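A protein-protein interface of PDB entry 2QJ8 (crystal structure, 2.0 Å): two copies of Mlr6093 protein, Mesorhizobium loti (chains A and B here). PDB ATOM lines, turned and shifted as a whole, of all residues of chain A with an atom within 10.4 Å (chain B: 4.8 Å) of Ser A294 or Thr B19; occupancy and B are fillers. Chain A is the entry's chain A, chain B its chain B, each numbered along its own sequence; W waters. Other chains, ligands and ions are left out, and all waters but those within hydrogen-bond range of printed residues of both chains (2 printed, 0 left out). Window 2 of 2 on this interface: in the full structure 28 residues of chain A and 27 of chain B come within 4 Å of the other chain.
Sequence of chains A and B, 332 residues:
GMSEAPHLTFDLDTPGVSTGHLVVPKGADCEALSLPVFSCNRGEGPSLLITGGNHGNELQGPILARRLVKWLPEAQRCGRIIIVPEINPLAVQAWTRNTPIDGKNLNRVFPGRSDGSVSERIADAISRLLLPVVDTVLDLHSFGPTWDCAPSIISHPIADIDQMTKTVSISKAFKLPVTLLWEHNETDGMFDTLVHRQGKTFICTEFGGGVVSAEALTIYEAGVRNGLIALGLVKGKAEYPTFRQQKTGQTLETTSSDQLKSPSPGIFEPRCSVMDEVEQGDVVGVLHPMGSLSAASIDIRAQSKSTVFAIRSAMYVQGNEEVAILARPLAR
Pro A289 touches none of the printed residues of chain B. Printed residues of chain B within 4 Å of Leu A293: Val B37 (3.7 Å), Phe B38 (3.7 Å) and Lys B70 (3.3 Å). Of chain B, only Thr B19 (3.6 Å) and Lys B70 (3.97 Å) come within 4 Å of Ser A294. Thr B19 touches one residue of chain A. Of the printed residues of chain A, His B21 touches Gly A291 (2.7 Å). Of the printed residues of chain A, Phe B38 touches Leu A293 (3.7 Å). The nearest printed residue of chain B that does not touch Ser A294 is Gly B20 (6.6 Å). The nearest residue of chain A that does not touch Thr B19 is Leu A293 (4.2 Å). The nearest printed residue of chain A that does not touch His B21 is Ser A292 (4.6 Å).
OG of Ser A292 lies within hydrogen-bond range of OG of Ser A294 (2.7 Å). O of Gly B20 sits at hydrogen-bond distance from N of Val B37 (2.7 Å).
Water W2 bridges N of Leu A293 (3.1 Å) and O of Gly B20 (3.1 Å). Water W1 bridges OG of Ser A294 (3.2 Å) and OG1 of Thr B19 (3.2 Å).
NZ of Lys B70 is in hydrogen-bond range of O of Leu A293, at 3.3 Å. NE2 of His B21 lies within hydrogen-bond range of O of Gly A291 (2.7 Å).
Of the 11 printed residues of chain A, 3 touch a printed residue of chain B. Printed residues of chain A that touch a printed residue of chain B: Gly A291, Leu A293 and Ser A294. Hydrophobic or aromatic side chains of chain A within 4 Å of the printed part of chain B: Leu A293. Of the 9 printed residues of chain B, 5 touch a printed residue of chain A. Hydrophobic or aromatic side chains of chain B within 4 Å of the printed part of chain A: His B21 and Phe B38. Among the printed residues, no Asp or Glu carboxylate lies within 4 Å of a Lys or Arg side-chain nitrogen of the other chain.
No position is printed for both chains.
Among the printed residues, merely in contact across the chains: Leu A293 with Val B37, Leu A293 with Phe B38, Ser A294 with Thr B19 and Ser A294 with Lys B70.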
ATOM      1  N   HIS A 288       6.070   9.610  27.444  1.00  0.00           N
ATOM      2  CA  HIS A 288       7.180  10.499  27.207  1.00  0.00           C
ATOM      3  C   HIS A 288       7.372  11.333  28.480  1.00  0.00           C
ATOM      4  O   HIS A 288       6.438  12.035  28.871  1.00  0.00           O
ATOM      5  CB  HIS A 288       6.840  11.419  26.030  1.00  0.00           C
ATOM      6  CG  HIS A 288       6.538  10.691  24.756  1.00  0.00           C
ATOM      7  ND1 HIS A 288       7.521  10.145  23.962  1.00  0.00           N
ATOM      8  CD2 HIS A 288       5.367  10.441  24.126  1.00  0.00           C
ATOM      9  CE1 HIS A 288       6.968   9.574  22.907  1.00  0.00           C
ATOM     10  NE2 HIS A 288       5.664   9.747  22.979  1.00  0.00           N
ATOM     11  N   PRO A 289       8.575  11.319  29.093  1.00  0.00           N
ATOM     12  CA  PRO A 289       8.815  12.100  30.328  1.00  0.00           C
ATOM     13  C   PRO A 289       8.720  13.613  30.128  1.00  0.00           C
ATOM     14  O   PRO A 289       9.314  14.136  29.187  1.00  0.00           O
ATOM     15  CB  PRO A 289      10.238  11.709  30.699  1.00  0.00           C
ATOM     16  CG  PRO A 289      10.877  11.381  29.417  1.00  0.00           C
ATOM     17  CD  PRO A 289       9.810  10.647  28.661  1.00  0.00           C
ATOM     18  N   MET A 290       8.032  14.302  31.044  1.00  0.00           N
ATOM     19  CA  MET A 290       7.774  15.754  30.915  1.00  0.00           C
ATOM     20  C   MET A 290       8.927  16.756  31.084  1.00  0.00           C
ATOM     21  O   MET A 290       8.919  17.810  30.420  1.00  0.00           O
ATOM     22  CB  MET A 290       6.600  16.165  31.827  1.00  0.00           C
ATOM     23  CG  MET A 290       5.245  15.816  31.248  1.00  0.00           C
ATOM     24  SD  MET A 290       3.873  15.482  32.614  1.00  0.00           S
ATOM     25  N   GLY A 291       9.887  16.471  31.947  1.00  0.00           N
ATOM     26  CA  GLY A 291      10.984  17.425  32.187  1.00  0.00           C
ATOM     27  C   GLY A 291      12.291  17.232  31.463  1.00  0.00           C
ATOM     28  O   GLY A 291      13.276  17.846  31.849  1.00  0.00           O
ATOM     29  N   SER A 292      12.314  16.386  30.430  1.00  0.00           N
ATOM     30  CA  SER A 292      13.555  16.058  29.730  1.00  0.00           C
ATOM     31  C   SER A 292      13.358  15.563  28.295  1.00  0.00           C
ATOM     32  O   SER A 292      12.414  14.816  28.008  1.00  0.00           O
ATOM     33  CB  SER A 292      14.303  14.976  30.516  1.00  0.00           C
ATOM     34  OG  SER A 292      15.578  14.715  29.968  1.00  0.00           O
ATOM     35  N   LEU A 293      14.252  16.016  27.412  1.00  0.00           N
ATOM     36  CA  LEU A 293      14.303  15.580  26.018  1.00  0.00           C
ATOM     37  C   LEU A 293      15.430  14.582  25.799  1.00  0.00           C
ATOM     38  O   LEU A 293      15.515  13.993  24.729  1.00  0.00           O
ATOM     39  CB  LEU A 293      14.399  16.791  25.065  1.00  0.00           C
ATOM     40  CG  LEU A 293      13.134  17.643  25.044  1.00  0.00           C
ATOM     41  CD1 LEU A 293      13.257  18.922  24.207  1.00  0.00           C
ATOM     42  CD2 LEU A 293      11.960  16.822  24.550  1.00  0.00           C
ATOM     43  N   SER A 294      16.270  14.370  26.813  1.00  0.00           N
ATOM     44  CA  SER A 294      17.343  13.384  26.781  1.00  0.00           C
ATOM     45  C   SER A 294      16.877  12.019  27.284  1.00  0.00           C
ATOM     46  O   SER A 294      17.380  10.994  26.808  1.00  0.00           O
ATOM     47  CB  SER A 294      18.519  13.865  27.632  1.00  0.00           C
ATOM     48  OG  SER A 294      18.030  14.372  28.859  1.00  0.00           O
ATOM     49  N   ALA A 295      15.935  12.002  28.238  1.00  0.00           N
ATOM     50  CA  ALA A 295      15.418  10.755  28.805  1.00  0.00           C
ATOM     51  C   ALA A 295      14.599   9.923  27.799  1.00  0.00           C
ATOM     52  O   ALA A 295      13.907  10.471  26.938  1.00  0.00           O
ATOM     53  CB  ALA A 295      14.592  11.047  30.050  1.00  0.00           C
ATOM     54  N   ALA A 296      14.702   8.597  27.922  1.00  0.00           N
ATOM     55  CA  ALA A 296      13.989   7.642  27.057  1.00  0.00           C
ATOM     56  C   ALA A 296      12.515   7.540  27.449  1.00  0.00           C
ATOM     57  O   ALA A 296      12.144   7.802  28.602  1.00  0.00           O
ATOM     58  CB  ALA A 296      14.652   6.227  27.126  1.00  0.00           C
ATOM     59  N   SER A 297      11.687   7.211  26.461  1.00  0.00           N
ATOM     60  CA  SER A 297      10.259   7.014  26.672  1.00  0.00           C
ATOM     61  C   SER A 297      10.021   5.614  27.255  1.00  0.00           C
ATOM     62  O   SER A 297      10.842   4.688  27.046  1.00  0.00           O
ATOM     63  CB  SER A 297       9.480   7.193  25.368  1.00  0.00           C
ATOM     64  OG  SER A 297       9.905   6.267  24.388  1.00  0.00           O
ATOM     65  N   ILE A 298       8.902   5.473  27.969  1.00  0.00           N
ATOM     66  CA  ILE A 298       8.493   4.243  28.648  1.00  0.00           C
ATOM     67  C   ILE A 298       7.374   3.565  27.878  1.00  0.00           C
ATOM     68  O   ILE A 298       6.374   4.195  27.579  1.00  0.00           O
ATOM     69  CB  ILE A 298       7.989   4.591  30.092  1.00  0.00           C
ATOM     70  CG1 ILE A 298       9.150   5.109  30.965  1.00  0.00           C
ATOM     71  CG2 ILE A 298       7.282   3.407  30.774  1.00  0.00           C
ATOM     72  CD1 ILE A 298       8.714   5.854  32.218  1.00  0.00           C
ATOM     73  N   PHE B  10      22.210  25.731  28.591  1.00  0.00           N
ATOM     74  CA  PHE B  10      23.348  25.372  27.768  1.00  0.00           C
ATOM     75  C   PHE B  10      23.589  26.511  26.790  1.00  0.00           C
ATOM     76  O   PHE B  10      22.752  27.406  26.646  1.00  0.00           O
ATOM     77  CB  PHE B  10      23.079  24.055  27.015  1.00  0.00           C
ATOM     78  CG  PHE B  10      21.923  24.119  26.047  1.00  0.00           C
ATOM     79  CD1 PHE B  10      20.621  23.956  26.495  1.00  0.00           C
ATOM     80  CD2 PHE B  10      22.142  24.335  24.697  1.00  0.00           C
ATOM     81  CE1 PHE B  10      19.539  24.019  25.620  1.00  0.00           C
ATOM     82  CE2 PHE B  10      21.069  24.392  23.807  1.00  0.00           C
ATOM     83  CZ  PHE B  10      19.762  24.231  24.275  1.00  0.00           C
ATOM     84  N   VAL B  17      24.475  18.351  19.159  1.00  0.00           N
ATOM     85  CA  VAL B  17      23.229  18.232  19.895  1.00  0.00           C
ATOM     86  C   VAL B  17      23.383  18.639  21.355  1.00  0.00           C
ATOM     87  O   VAL B  17      24.352  18.248  21.996  1.00  0.00           O
ATOM     88  CB  VAL B  17      22.698  16.774  19.810  1.00  0.00           C
ATOM     89  CG1 VAL B  17      21.427  16.593  20.659  1.00  0.00           C
ATOM     90  CG2 VAL B  17      22.443  16.413  18.346  1.00  0.00           C
ATOM     91  N   SER B  18      22.429  19.437  21.851  1.00  0.00           N
ATOM     92  CA  SER B  18      22.334  19.850  23.263  1.00  0.00           C
ATOM     93  C   SER B  18      20.853  19.734  23.655  1.00  0.00           C
ATOM     94  O   SER B  18      19.960  19.927  22.815  1.00  0.00           O
ATOM     95  CB  SER B  18      22.809  21.291  23.493  1.00  0.00           C
ATOM     96  OG  SER B  18      24.156  21.500  23.115  1.00  0.00           O
ATOM     97  N   THR B  19      20.621  19.352  24.904  1.00  0.00           N
ATOM     98  CA  THR B  19      19.302  19.251  25.490  1.00  0.00           C
ATOM     99  C   THR B  19      19.434  19.947  26.835  1.00  0.00           C
ATOM    100  O   THR B  19      20.436  19.806  27.524  1.00  0.00           O
ATOM    101  CB  THR B  19      18.771  17.783  25.692  1.00  0.00           C
ATOM    102  OG1 THR B  19      19.712  17.012  26.443  1.00  0.00           O
ATOM    103  CG2 THR B  19      18.508  17.094  24.378  1.00  0.00           C
ATOM    104  N   GLY B  20      18.423  20.712  27.203  1.00  0.00           N
ATOM    105  CA  GLY B  20      18.457  21.433  28.451  1.00  0.00           C
ATOM    106  C   GLY B  20      17.113  22.068  28.632  1.00  0.00           C
ATOM    107  O   GLY B  20      16.113  21.532  28.142  1.00  0.00           O
ATOM    108  N   HIS B  21      17.091  23.222  29.286  1.00  0.00           N
ATOM    109  CA  HIS B  21      15.865  23.923  29.611  1.00  0.00           C
ATOM    110  C   HIS B  21      15.951  25.427  29.393  1.00  0.00           C
ATOM    111  O   HIS B  21      17.022  26.004  29.430  1.00  0.00           O
ATOM    112  CB  HIS B  21      15.492  23.670  31.086  1.00  0.00           C
ATOM    113  CG  HIS B  21      15.325  22.220  31.414  1.00  0.00           C
ATOM    114  ND1 HIS B  21      16.397  21.397  31.681  1.00  0.00           N
ATOM    115  CD2 HIS B  21      14.231  21.433  31.443  1.00  0.00           C
ATOM    116  CE1 HIS B  21      15.964  20.169  31.888  1.00  0.00           C
ATOM    117  NE2 HIS B  21      14.654  20.164  31.751  1.00  0.00           N
ATOM    118  N   VAL B  37      14.379  22.065  26.104  1.00  0.00           N
ATOM    119  CA  VAL B  37      14.784  22.548  24.789  1.00  0.00           C
ATOM    120  C   VAL B  37      15.830  21.614  24.206  1.00  0.00           C
ATOM    121  O   VAL B  37      16.722  21.163  24.903  1.00  0.00           O
ATOM    122  CB  VAL B  37      15.391  23.971  24.871  1.00  0.00           C
ATOM    123  CG1 VAL B  37      15.858  24.463  23.487  1.00  0.00           C
ATOM    124  CG2 VAL B  37      14.405  24.932  25.446  1.00  0.00           C
ATOM    125  N   PHE B  38      15.689  21.324  22.917  1.00  0.00           N
ATOM    126  CA  PHE B  38      16.644  20.582  22.120  1.00  0.00           C
ATOM    127  C   PHE B  38      17.241  21.553  21.111  1.00  0.00           C
ATOM    128  O   PHE B  38      16.532  22.358  20.548  1.00  0.00           O
ATOM    129  CB  PHE B  38      15.917  19.482  21.353  1.00  0.00           C
ATOM    130  CG  PHE B  38      16.710  18.871  20.248  1.00  0.00           C
ATOM    131  CD1 PHE B  38      17.509  17.778  20.482  1.00  0.00           C
ATOM    132  CD2 PHE B  38      16.597  19.346  18.932  1.00  0.00           C
ATOM    133  CE1 PHE B  38      18.200  17.202  19.444  1.00  0.00           C
ATOM    134  CE2 PHE B  38      17.291  18.761  17.926  1.00  0.00           C
ATOM    135  CZ  PHE B  38      18.095  17.679  18.202  1.00  0.00           C
ATOM    136  N   LYS B  70      14.493  13.006  18.243  1.00  0.00           N
ATOM    137  CA  LYS B  70      15.201  11.713  18.132  1.00  0.00           C
ATOM    138  C   LYS B  70      15.837  11.437  16.744  1.00  0.00           C
ATOM    139  O   LYS B  70      16.888  10.803  16.644  1.00  0.00           O
ATOM    140  CB  LYS B  70      14.255  10.570  18.538  1.00  0.00           C
ATOM    141  CG  LYS B  70      13.736  10.689  19.987  1.00  0.00           C
ATOM    142  CD  LYS B  70      14.862  10.451  21.031  1.00  0.00           C
ATOM    143  CE  LYS B  70      14.712  11.253  22.343  1.00  0.00           C
ATOM    144  NZ  LYS B  70      16.014  11.217  23.092  1.00  0.00           N
HETATM  145  O   HOH W   1      18.292  17.533  29.288  1.00  0.00           O
HETATM  146  O   HOH W   2      15.941  18.468  28.104  1.00  0.00           O
